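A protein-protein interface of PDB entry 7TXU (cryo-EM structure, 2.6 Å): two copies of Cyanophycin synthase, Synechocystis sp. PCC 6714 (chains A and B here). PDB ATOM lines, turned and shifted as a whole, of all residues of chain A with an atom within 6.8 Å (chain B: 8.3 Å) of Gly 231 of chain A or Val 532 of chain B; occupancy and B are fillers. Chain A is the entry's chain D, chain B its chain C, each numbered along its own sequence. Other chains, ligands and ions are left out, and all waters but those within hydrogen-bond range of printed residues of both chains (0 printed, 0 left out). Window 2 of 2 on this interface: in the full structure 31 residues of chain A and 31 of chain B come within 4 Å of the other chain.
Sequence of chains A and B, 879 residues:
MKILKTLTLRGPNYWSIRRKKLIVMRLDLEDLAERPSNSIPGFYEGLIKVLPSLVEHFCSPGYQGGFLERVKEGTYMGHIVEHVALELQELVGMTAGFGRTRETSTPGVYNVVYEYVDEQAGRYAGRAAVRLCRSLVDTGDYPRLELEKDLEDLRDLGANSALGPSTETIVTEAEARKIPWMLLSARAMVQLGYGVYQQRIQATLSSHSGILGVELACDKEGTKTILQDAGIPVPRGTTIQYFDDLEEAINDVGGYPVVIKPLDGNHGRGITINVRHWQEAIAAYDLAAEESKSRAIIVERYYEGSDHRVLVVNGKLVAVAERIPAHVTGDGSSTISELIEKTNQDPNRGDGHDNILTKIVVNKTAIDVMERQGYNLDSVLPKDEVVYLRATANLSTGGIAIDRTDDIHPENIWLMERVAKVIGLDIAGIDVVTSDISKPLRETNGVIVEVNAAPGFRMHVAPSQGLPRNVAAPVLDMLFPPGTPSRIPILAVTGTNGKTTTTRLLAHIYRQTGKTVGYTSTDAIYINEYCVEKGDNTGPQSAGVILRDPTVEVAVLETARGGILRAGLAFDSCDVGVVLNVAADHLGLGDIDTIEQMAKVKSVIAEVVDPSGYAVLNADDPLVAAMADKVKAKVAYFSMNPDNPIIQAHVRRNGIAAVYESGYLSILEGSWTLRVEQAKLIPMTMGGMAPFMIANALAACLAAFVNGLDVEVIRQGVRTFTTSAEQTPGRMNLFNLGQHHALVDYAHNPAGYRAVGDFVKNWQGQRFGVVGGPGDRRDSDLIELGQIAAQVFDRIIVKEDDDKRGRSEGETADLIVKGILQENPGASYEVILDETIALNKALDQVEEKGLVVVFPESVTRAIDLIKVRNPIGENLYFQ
The backbone NH (N) of Val 532 of chain B is in hydrogen-bond range of the backbone carbonyl oxygen (O) of Ile 525 of chain B (2.8 Å).
The side-chain sulfur (SG) of Cys 531 of chain B is in hydrogen-bond range of the backbone carbonyl oxygen (O) of Glu 533 of chain B, 3.3 Å away.
O of Glu 533 of chain B is in hydrogen-bond range of N of Ile 525 of chain B (2.9 Å).
The backbone carbonyl oxygen (O) of Ala 230 of chain A lies within hydrogen-bond range of the guanidinium group (NH2) of Arg 418 of chain A (3.0 Å).
Of the 11 printed residues of chain A, 5 touch a printed residue of chain B.
Hydrophobic or aromatic side chains of chain A that line the printed part of chain B: Trp 414.
Hydrophobic or aromatic side chains of chain B that line the printed part of chain A: Tyr 530, Val 532 and Val 545.
Along chain B the printed residues that touch a printed residue of chain A span positions 530 to 549.
No position is printed for both chains.
Printed residues of chain B within 4 Å of Asp 229 of chain A: Val 545 (3.9 Å).
Of the printed residues of chain B, Gly 231 of chain A touches Val 532 (3.7 Å) and Glu 533 (3.96 Å).
Printed residues of chain B within 4 Å of Trp 414 of chain A: Tyr 530 (3.6 Å).
Of the printed residues of chain B, Arg 418 of chain A touches Val 532 and Asp 549.
Val 532 of chain B touches just these residues of chain A: Ala 230, Gly 231 and Arg 418.
Gly 535 of chain B touches none of the printed residues of chain A.
Of the printed residues of chain A, Val 545 of chain B touches Asp 229 (3.9 Å).
Among the printed residues, pairs that only touch across the chains: Arg 418 of chain A with Val 532 of chain B, Ala 230 of chain A with Val 532 of chain B, Trp 414 of chain A with Tyr 530 of chain B, Gly 231 of chain A with Val 532 of chain B, Asp 229 of chain A with Val 545 of chain B and Gly 231 of chain A with Glu 533 of chain B.
OD2 of Asp 549 of chain B is in salt-bridge range of NH1 of Arg 418 of chain A.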
ATOM      1  N   ILE A 226     -16.164   9.761 -13.253  1.00  0.00           N
ATOM      2  CA  ILE A 226     -16.538  10.232 -11.936  1.00  0.00           C
ATOM      3  C   ILE A 226     -15.452  11.067 -11.319  1.00  0.00           C
ATOM      4  O   ILE A 226     -15.749  12.063 -10.668  1.00  0.00           O
ATOM      5  CB  ILE A 226     -16.890   9.041 -11.017  1.00  0.00           C
ATOM      6  CG1 ILE A 226     -18.143   8.309 -11.507  1.00  0.00           C
ATOM      7  CG2 ILE A 226     -17.033   9.452  -9.582  1.00  0.00           C
ATOM      8  CD1 ILE A 226     -19.433   9.079 -11.527  1.00  0.00           C
ATOM      9  N   LEU A 227     -14.201  10.659 -11.454  1.00  0.00           N
ATOM     10  CA  LEU A 227     -13.148  11.442 -10.862  1.00  0.00           C
ATOM     11  C   LEU A 227     -12.874  12.742 -11.577  1.00  0.00           C
ATOM     12  O   LEU A 227     -12.686  13.764 -10.920  1.00  0.00           O
ATOM     13  CB  LEU A 227     -11.852  10.636 -10.800  1.00  0.00           C
ATOM     14  CG  LEU A 227     -11.807   9.424  -9.868  1.00  0.00           C
ATOM     15  CD1 LEU A 227     -10.505   8.745 -10.062  1.00  0.00           C
ATOM     16  CD2 LEU A 227     -11.985   9.814  -8.412  1.00  0.00           C
ATOM     17  N   GLN A 228     -12.930  12.795 -12.901  1.00  0.00           N
ATOM     18  CA  GLN A 228     -12.609  14.081 -13.498  1.00  0.00           C
ATOM     19  C   GLN A 228     -13.704  15.111 -13.256  1.00  0.00           C
ATOM     20  O   GLN A 228     -13.416  16.300 -13.138  1.00  0.00           O
ATOM     21  CB  GLN A 228     -12.243  13.955 -14.960  1.00  0.00           C
ATOM     22  CG  GLN A 228     -13.297  13.630 -15.869  1.00  0.00           C
ATOM     23  CD  GLN A 228     -12.727  13.379 -17.228  1.00  0.00           C
ATOM     24  OE1 GLN A 228     -11.810  12.552 -17.399  1.00  0.00           O
ATOM     25  NE2 GLN A 228     -13.242  14.092 -18.206  1.00  0.00           N
ATOM     26  N   ASP A 229     -14.929  14.673 -13.009  1.00  0.00           N
ATOM     27  CA  ASP A 229     -16.016  15.585 -12.679  1.00  0.00           C
ATOM     28  C   ASP A 229     -15.860  16.190 -11.286  1.00  0.00           C
ATOM     29  O   ASP A 229     -16.563  17.129 -10.928  1.00  0.00           O
ATOM     30  CB  ASP A 229     -17.369  14.893 -12.725  1.00  0.00           C
ATOM     31  CG  ASP A 229     -17.884  14.575 -14.106  1.00  0.00           C
ATOM     32  OD1 ASP A 229     -17.370  15.085 -15.078  1.00  0.00           O
ATOM     33  OD2 ASP A 229     -18.840  13.838 -14.183  1.00  0.00           O
ATOM     34  N   ALA A 230     -14.999  15.599 -10.459  1.00  0.00           N
ATOM     35  CA  ALA A 230     -14.747  16.018  -9.103  1.00  0.00           C
ATOM     36  C   ALA A 230     -13.507  16.889  -9.031  1.00  0.00           C
ATOM     37  O   ALA A 230     -13.087  17.288  -7.940  1.00  0.00           O
ATOM     38  CB  ALA A 230     -14.587  14.801  -8.219  1.00  0.00           C
ATOM     39  N   GLY A 231     -12.876  17.143 -10.184  1.00  0.00           N
ATOM     40  CA  GLY A 231     -11.658  17.923 -10.236  1.00  0.00           C
ATOM     41  C   GLY A 231     -10.378  17.157  -9.900  1.00  0.00           C
ATOM     42  O   GLY A 231      -9.400  17.765  -9.479  1.00  0.00           O
ATOM     43  N   ILE A 232     -10.373  15.841 -10.048  1.00  0.00           N
ATOM     44  CA  ILE A 232      -9.219  15.012  -9.732  1.00  0.00           C
ATOM     45  C   ILE A 232      -8.406  14.727 -11.009  1.00  0.00           C
ATOM     46  O   ILE A 232      -9.006  14.409 -12.029  1.00  0.00           O
ATOM     47  CB  ILE A 232      -9.735  13.752  -9.029  1.00  0.00           C
ATOM     48  CG1 ILE A 232     -10.411  14.213  -7.689  1.00  0.00           C
ATOM     49  CG2 ILE A 232      -8.662  12.725  -8.847  1.00  0.00           C
ATOM     50  CD1 ILE A 232     -11.232  13.206  -6.959  1.00  0.00           C
ATOM     51  N   PRO A 233      -7.061  14.943 -11.043  1.00  0.00           N
ATOM     52  CA  PRO A 233      -6.212  14.714 -12.213  1.00  0.00           C
ATOM     53  C   PRO A 233      -6.093  13.254 -12.627  1.00  0.00           C
ATOM     54  O   PRO A 233      -5.643  12.419 -11.848  1.00  0.00           O
ATOM     55  CB  PRO A 233      -4.865  15.244 -11.738  1.00  0.00           C
ATOM     56  CG  PRO A 233      -4.910  15.162 -10.241  1.00  0.00           C
ATOM     57  CD  PRO A 233      -6.339  15.414  -9.864  1.00  0.00           C
ATOM     58  N   TRP A 414      -4.477  14.695   1.441  1.00  0.00           N
ATOM     59  CA  TRP A 414      -5.853  15.144   1.307  1.00  0.00           C
ATOM     60  C   TRP A 414      -6.492  14.651   0.020  1.00  0.00           C
ATOM     61  O   TRP A 414      -7.619  14.149   0.035  1.00  0.00           O
ATOM     62  CB  TRP A 414      -5.891  16.672   1.393  1.00  0.00           C
ATOM     63  CG  TRP A 414      -7.206  17.299   1.072  1.00  0.00           C
ATOM     64  CD1 TRP A 414      -8.249  17.463   1.884  1.00  0.00           C
ATOM     65  CD2 TRP A 414      -7.590  17.890  -0.173  1.00  0.00           C
ATOM     66  NE1 TRP A 414      -9.251  18.081   1.232  1.00  0.00           N
ATOM     67  CE2 TRP A 414      -8.861  18.346  -0.021  1.00  0.00           C
ATOM     68  CE3 TRP A 414      -6.952  18.061  -1.385  1.00  0.00           C
ATOM     69  CZ2 TRP A 414      -9.524  18.957  -1.025  1.00  0.00           C
ATOM     70  CZ3 TRP A 414      -7.613  18.672  -2.393  1.00  0.00           C
ATOM     71  CH2 TRP A 414      -8.872  19.110  -2.219  1.00  0.00           C
ATOM     72  N   LEU A 415      -5.780  14.758  -1.091  1.00  0.00           N
ATOM     73  CA  LEU A 415      -6.325  14.314  -2.347  1.00  0.00           C
ATOM     74  C   LEU A 415      -6.606  12.820  -2.377  1.00  0.00           C
ATOM     75  O   LEU A 415      -7.641  12.413  -2.894  1.00  0.00           O
ATOM     76  CB  LEU A 415      -5.368  14.658  -3.472  1.00  0.00           C
ATOM     77  CG  LEU A 415      -5.777  14.273  -4.898  1.00  0.00           C
ATOM     78  CD1 LEU A 415      -7.051  14.958  -5.312  1.00  0.00           C
ATOM     79  CD2 LEU A 415      -4.686  14.631  -5.800  1.00  0.00           C
ATOM     80  N   ARG A 418      -9.771  11.953  -0.529  1.00  0.00           N
ATOM     81  CA  ARG A 418     -10.931  12.413  -1.269  1.00  0.00           C
ATOM     82  C   ARG A 418     -11.266  11.435  -2.394  1.00  0.00           C
ATOM     83  O   ARG A 418     -12.439  11.151  -2.606  1.00  0.00           O
ATOM     84  CB  ARG A 418     -10.719  13.838  -1.791  1.00  0.00           C
ATOM     85  CG  ARG A 418     -12.006  14.533  -2.258  1.00  0.00           C
ATOM     86  CD  ARG A 418     -11.884  16.034  -2.357  1.00  0.00           C
ATOM     87  NE  ARG A 418     -11.186  16.529  -3.518  1.00  0.00           N
ATOM     88  CZ  ARG A 418     -11.771  16.794  -4.722  1.00  0.00           C
ATOM     89  NH1 ARG A 418     -13.043  16.615  -4.932  1.00  0.00           N
ATOM     90  NH2 ARG A 418     -11.072  17.257  -5.726  1.00  0.00           N
ATOM     91  N   GLY B 518     -16.773  24.130   1.960  1.00  0.00           N
ATOM     92  CA  GLY B 518     -16.493  24.231   0.556  1.00  0.00           C
ATOM     93  C   GLY B 518     -17.091  25.505   0.031  1.00  0.00           C
ATOM     94  O   GLY B 518     -18.147  25.924   0.499  1.00  0.00           O
ATOM     95  N   TYR B 519     -16.449  26.115  -0.940  1.00  0.00           N
ATOM     96  CA  TYR B 519     -17.021  27.311  -1.513  1.00  0.00           C
ATOM     97  C   TYR B 519     -16.612  27.545  -2.940  1.00  0.00           C
ATOM     98  O   TYR B 519     -15.558  27.102  -3.402  1.00  0.00           O
ATOM     99  CB  TYR B 519     -16.710  28.542  -0.649  1.00  0.00           C
ATOM    100  CG  TYR B 519     -15.318  29.000  -0.539  1.00  0.00           C
ATOM    101  CD1 TYR B 519     -14.495  28.459   0.387  1.00  0.00           C
ATOM    102  CD2 TYR B 519     -14.878  30.015  -1.344  1.00  0.00           C
ATOM    103  CE1 TYR B 519     -13.243  28.921   0.506  1.00  0.00           C
ATOM    104  CE2 TYR B 519     -13.628  30.473  -1.228  1.00  0.00           C
ATOM    105  CZ  TYR B 519     -12.811  29.936  -0.304  1.00  0.00           C
ATOM    106  OH  TYR B 519     -11.541  30.399  -0.169  1.00  0.00           O
ATOM    107  N   ALA B 524     -11.760  30.464  -8.165  1.00  0.00           N
ATOM    108  CA  ALA B 524     -11.549  29.019  -8.003  1.00  0.00           C
ATOM    109  C   ALA B 524     -12.640  28.323  -7.160  1.00  0.00           C
ATOM    110  O   ALA B 524     -13.481  28.970  -6.534  1.00  0.00           O
ATOM    111  CB  ALA B 524     -10.209  28.781  -7.361  1.00  0.00           C
ATOM    112  N   ILE B 525     -12.569  26.986  -7.110  1.00  0.00           N
ATOM    113  CA  ILE B 525     -13.362  26.153  -6.193  1.00  0.00           C
ATOM    114  C   ILE B 525     -12.433  25.631  -5.122  1.00  0.00           C
ATOM    115  O   ILE B 525     -11.430  25.007  -5.457  1.00  0.00           O
ATOM    116  CB  ILE B 525     -14.013  24.928  -6.860  1.00  0.00           C
ATOM    117  CG1 ILE B 525     -14.921  25.364  -7.913  1.00  0.00           C
ATOM    118  CG2 ILE B 525     -14.725  24.088  -5.830  1.00  0.00           C
ATOM    119  CD1 ILE B 525     -15.479  24.264  -8.781  1.00  0.00           C
ATOM    120  N   TYR B 526     -12.773  25.859  -3.850  1.00  0.00           N
ATOM    121  CA  TYR B 526     -11.964  25.420  -2.713  1.00  0.00           C
ATOM    122  C   TYR B 526     -12.661  24.571  -1.690  1.00  0.00           C
ATOM    123  O   TYR B 526     -13.848  24.751  -1.425  1.00  0.00           O
ATOM    124  CB  TYR B 526     -11.462  26.589  -1.903  1.00  0.00           C
ATOM    125  CG  TYR B 526     -10.529  27.425  -2.524  1.00  0.00           C
ATOM    126  CD1 TYR B 526     -10.940  28.443  -3.276  1.00  0.00           C
ATOM    127  CD2 TYR B 526      -9.223  27.203  -2.315  1.00  0.00           C
ATOM    128  CE1 TYR B 526     -10.036  29.240  -3.835  1.00  0.00           C
ATOM    129  CE2 TYR B 526      -8.312  27.988  -2.881  1.00  0.00           C
ATOM    130  CZ  TYR B 526      -8.715  29.007  -3.646  1.00  0.00           C
ATOM    131  OH  TYR B 526      -7.794  29.832  -4.229  1.00  0.00           O
ATOM    132  N   ILE B 527     -11.902  23.665  -1.079  1.00  0.00           N
ATOM    133  CA  ILE B 527     -12.360  22.941   0.102  1.00  0.00           C
ATOM    134  C   ILE B 527     -11.310  23.047   1.197  1.00  0.00           C
ATOM    135  O   ILE B 527     -10.210  22.539   1.028  1.00  0.00           O
ATOM    136  CB  ILE B 527     -12.659  21.463  -0.190  1.00  0.00           C
ATOM    137  CG1 ILE B 527     -13.729  21.369  -1.275  1.00  0.00           C
ATOM    138  CG2 ILE B 527     -13.120  20.782   1.094  1.00  0.00           C
ATOM    139  CD1 ILE B 527     -14.005  20.014  -1.794  1.00  0.00           C
ATOM    140  N   ASN B 528     -11.627  23.688   2.324  1.00  0.00           N
ATOM    141  CA  ASN B 528     -10.675  23.833   3.438  1.00  0.00           C
ATOM    142  C   ASN B 528      -9.305  24.312   3.035  1.00  0.00           C
ATOM    143  O   ASN B 528      -8.314  23.724   3.453  1.00  0.00           O
ATOM    144  CB  ASN B 528     -10.484  22.593   4.257  1.00  0.00           C
ATOM    145  CG  ASN B 528     -11.594  22.225   4.955  1.00  0.00           C
ATOM    146  OD1 ASN B 528     -12.514  23.040   5.149  1.00  0.00           O
ATOM    147  ND2 ASN B 528     -11.563  21.007   5.415  1.00  0.00           N
ATOM    148  N   GLU B 529      -9.236  25.345   2.242  1.00  0.00           N
ATOM    149  CA  GLU B 529      -7.976  25.928   1.757  1.00  0.00           C
ATOM    150  C   GLU B 529      -7.187  25.134   0.715  1.00  0.00           C
ATOM    151  O   GLU B 529      -6.103  25.560   0.327  1.00  0.00           O
ATOM    152  CB  GLU B 529      -7.009  26.176   2.932  1.00  0.00           C
ATOM    153  CG  GLU B 529      -7.563  27.063   4.051  1.00  0.00           C
ATOM    154  CD  GLU B 529      -6.616  27.232   5.178  1.00  0.00           C
ATOM    155  OE1 GLU B 529      -5.649  26.520   5.221  1.00  0.00           O
ATOM    156  OE2 GLU B 529      -6.859  28.071   6.016  1.00  0.00           O
ATOM    157  N   TYR B 530      -7.755  24.076   0.155  1.00  0.00           N
ATOM    158  CA  TYR B 530      -7.120  23.416  -0.966  1.00  0.00           C
ATOM    159  C   TYR B 530      -7.881  23.759  -2.211  1.00  0.00           C
ATOM    160  O   TYR B 530      -9.107  23.777  -2.224  1.00  0.00           O
ATOM    161  CB  TYR B 530      -7.077  21.923  -0.797  1.00  0.00           C
ATOM    162  CG  TYR B 530      -6.206  21.470   0.288  1.00  0.00           C
ATOM    163  CD1 TYR B 530      -4.864  21.461   0.110  1.00  0.00           C
ATOM    164  CD2 TYR B 530      -6.739  21.082   1.468  1.00  0.00           C
ATOM    165  CE1 TYR B 530      -4.049  21.051   1.110  1.00  0.00           C
ATOM    166  CE2 TYR B 530      -5.923  20.665   2.466  1.00  0.00           C
ATOM    167  CZ  TYR B 530      -4.572  20.652   2.276  1.00  0.00           C
ATOM    168  OH  TYR B 530      -3.746  20.236   3.280  1.00  0.00           O
ATOM    169  N   CYS B 531      -7.183  23.999  -3.287  1.00  0.00           N
ATOM    170  CA  CYS B 531      -7.862  24.343  -4.517  1.00  0.00           C
ATOM    171  C   CYS B 531      -8.224  23.102  -5.304  1.00  0.00           C
ATOM    172  O   CYS B 531      -7.391  22.225  -5.510  1.00  0.00           O
ATOM    173  CB  CYS B 531      -7.001  25.266  -5.339  1.00  0.00           C
ATOM    174  SG  CYS B 531      -7.765  25.804  -6.789  1.00  0.00           S
ATOM    175  N   VAL B 532      -9.478  23.012  -5.714  1.00  0.00           N
ATOM    176  CA  VAL B 532      -9.990  21.888  -6.469  1.00  0.00           C
ATOM    177  C   VAL B 532      -9.923  22.207  -7.959  1.00  0.00           C
ATOM    178  O   VAL B 532      -9.460  21.390  -8.749  1.00  0.00           O
ATOM    179  CB  VAL B 532     -11.435  21.589  -6.024  1.00  0.00           C
ATOM    180  CG1 VAL B 532     -12.033  20.504  -6.815  1.00  0.00           C
ATOM    181  CG2 VAL B 532     -11.442  21.232  -4.568  1.00  0.00           C
ATOM    182  N   GLU B 533     -10.418  23.378  -8.338  1.00  0.00           N
ATOM    183  CA  GLU B 533     -10.395  23.832  -9.737  1.00  0.00           C
ATOM    184  C   GLU B 533     -10.085  25.311  -9.770  1.00  0.00           C
ATOM    185  O   GLU B 533     -10.413  26.012  -8.823  1.00  0.00           O
ATOM    186  CB  GLU B 533     -11.710  23.599 -10.491  1.00  0.00           C
ATOM    187  CG  GLU B 533     -12.183  22.153 -10.577  1.00  0.00           C
ATOM    188  CD  GLU B 533     -13.356  21.935 -11.507  1.00  0.00           C
ATOM    189  OE1 GLU B 533     -13.610  22.802 -12.303  1.00  0.00           O
ATOM    190  OE2 GLU B 533     -13.986  20.901 -11.426  1.00  0.00           O
ATOM    191  N   LYS B 534      -9.492  25.810 -10.853  1.00  0.00           N
ATOM    192  CA  LYS B 534      -9.232  27.251 -10.999  1.00  0.00           C
ATOM    193  C   LYS B 534     -10.046  27.874 -12.122  1.00  0.00           C
ATOM    194  O   LYS B 534     -10.448  27.179 -13.053  1.00  0.00           O
ATOM    195  CB  LYS B 534      -7.762  27.513 -11.236  1.00  0.00           C
ATOM    196  CG  LYS B 534      -6.908  27.143 -10.080  1.00  0.00           C
ATOM    197  CD  LYS B 534      -5.463  27.453 -10.325  1.00  0.00           C
ATOM    198  CE  LYS B 534      -4.610  27.039  -9.131  1.00  0.00           C
ATOM    199  NZ  LYS B 534      -3.162  27.323  -9.351  1.00  0.00           N
ATOM    200  N   GLY B 535     -10.276  29.188 -12.053  1.00  0.00           N
ATOM    201  CA  GLY B 535     -11.009  29.903 -13.091  1.00  0.00           C
ATOM    202  C   GLY B 535     -12.366  30.359 -12.585  1.00  0.00           C
ATOM    203  O   GLY B 535     -12.698  30.175 -11.413  1.00  0.00           O
ATOM    204  N   ASN B 537     -15.601  30.014 -11.507  1.00  0.00           N
ATOM    205  CA  ASN B 537     -16.343  28.876 -11.109  1.00  0.00           C
ATOM    206  C   ASN B 537     -17.674  29.200 -10.539  1.00  0.00           C
ATOM    207  O   ASN B 537     -18.217  28.399  -9.796  1.00  0.00           O
ATOM    208  CB  ASN B 537     -15.511  27.987 -10.241  1.00  0.00           C
ATOM    209  CG  ASN B 537     -14.556  27.190 -11.076  1.00  0.00           C
ATOM    210  OD1 ASN B 537     -14.971  26.170 -11.612  1.00  0.00           O
ATOM    211  ND2 ASN B 537     -13.368  27.598 -11.239  1.00  0.00           N
ATOM    212  N   VAL B 545     -20.382  20.565  -7.841  1.00  0.00           N
ATOM    213  CA  VAL B 545     -19.158  19.896  -7.455  1.00  0.00           C
ATOM    214  C   VAL B 545     -19.124  19.864  -5.954  1.00  0.00           C
ATOM    215  O   VAL B 545     -18.801  18.846  -5.360  1.00  0.00           O
ATOM    216  CB  VAL B 545     -17.913  20.606  -8.018  1.00  0.00           C
ATOM    217  CG1 VAL B 545     -16.639  20.011  -7.472  1.00  0.00           C
ATOM    218  CG2 VAL B 545     -17.918  20.489  -9.491  1.00  0.00           C
ATOM    219  N   ILE B 546     -19.459  20.991  -5.336  1.00  0.00           N
ATOM    220  CA  ILE B 546     -19.488  21.066  -3.887  1.00  0.00           C
ATOM    221  C   ILE B 546     -20.612  20.226  -3.294  1.00  0.00           C
ATOM    222  O   ILE B 546     -20.388  19.485  -2.350  1.00  0.00           O
ATOM    223  CB  ILE B 546     -19.596  22.537  -3.403  1.00  0.00           C
ATOM    224  CG1 ILE B 546     -18.345  23.366  -3.800  1.00  0.00           C
ATOM    225  CG2 ILE B 546     -19.836  22.631  -1.903  1.00  0.00           C
ATOM    226  CD1 ILE B 546     -17.013  22.879  -3.243  1.00  0.00           C
ATOM    227  N   ARG B 548     -22.096  17.548  -4.442  1.00  0.00           N
ATOM    228  CA  ARG B 548     -21.875  16.121  -4.580  1.00  0.00           C
ATOM    229  C   ARG B 548     -20.664  15.609  -3.795  1.00  0.00           C
ATOM    230  O   ARG B 548     -20.417  14.410  -3.777  1.00  0.00           O
ATOM    231  CB  ARG B 548     -21.679  15.722  -6.024  1.00  0.00           C
ATOM    232  CG  ARG B 548     -22.884  15.824  -6.909  1.00  0.00           C
ATOM    233  CD  ARG B 548     -22.658  15.145  -8.179  1.00  0.00           C
ATOM    234  NE  ARG B 548     -21.563  15.718  -8.935  1.00  0.00           N
ATOM    235  CZ  ARG B 548     -21.647  16.716  -9.831  1.00  0.00           C
ATOM    236  NH1 ARG B 548     -22.802  17.274 -10.113  1.00  0.00           N
ATOM    237  NH2 ARG B 548     -20.550  17.137 -10.432  1.00  0.00           N
ATOM    238  N   ASP B 549     -19.880  16.490  -3.183  1.00  0.00           N
ATOM    239  CA  ASP B 549     -18.657  16.117  -2.494  1.00  0.00           C
ATOM    240  C   ASP B 549     -18.936  15.512  -1.118  1.00  0.00           C
ATOM    241  O   ASP B 549     -19.494  16.198  -0.267  1.00  0.00           O
ATOM    242  CB  ASP B 549     -17.714  17.297  -2.387  1.00  0.00           C
ATOM    243  CG  ASP B 549     -16.374  16.921  -1.801  1.00  0.00           C
ATOM    244  OD1 ASP B 549     -16.340  16.288  -0.757  1.00  0.00           O
ATOM    245  OD2 ASP B 549     -15.386  17.208  -2.406  1.00  0.00           O
ATOM    246  N   VAL B 552     -18.012  17.508   2.383  1.00  0.00           N
ATOM    247  CA  VAL B 552     -18.416  18.866   2.727  1.00  0.00           C
ATOM    248  C   VAL B 552     -19.560  18.958   3.722  1.00  0.00           C
ATOM    249  O   VAL B 552     -20.579  18.280   3.595  1.00  0.00           O
ATOM    250  CB  VAL B 552     -18.711  19.642   1.428  1.00  0.00           C
ATOM    251  CG1 VAL B 552     -19.251  20.997   1.701  1.00  0.00           C
ATOM    252  CG2 VAL B 552     -17.414  19.790   0.646  1.00  0.00           C
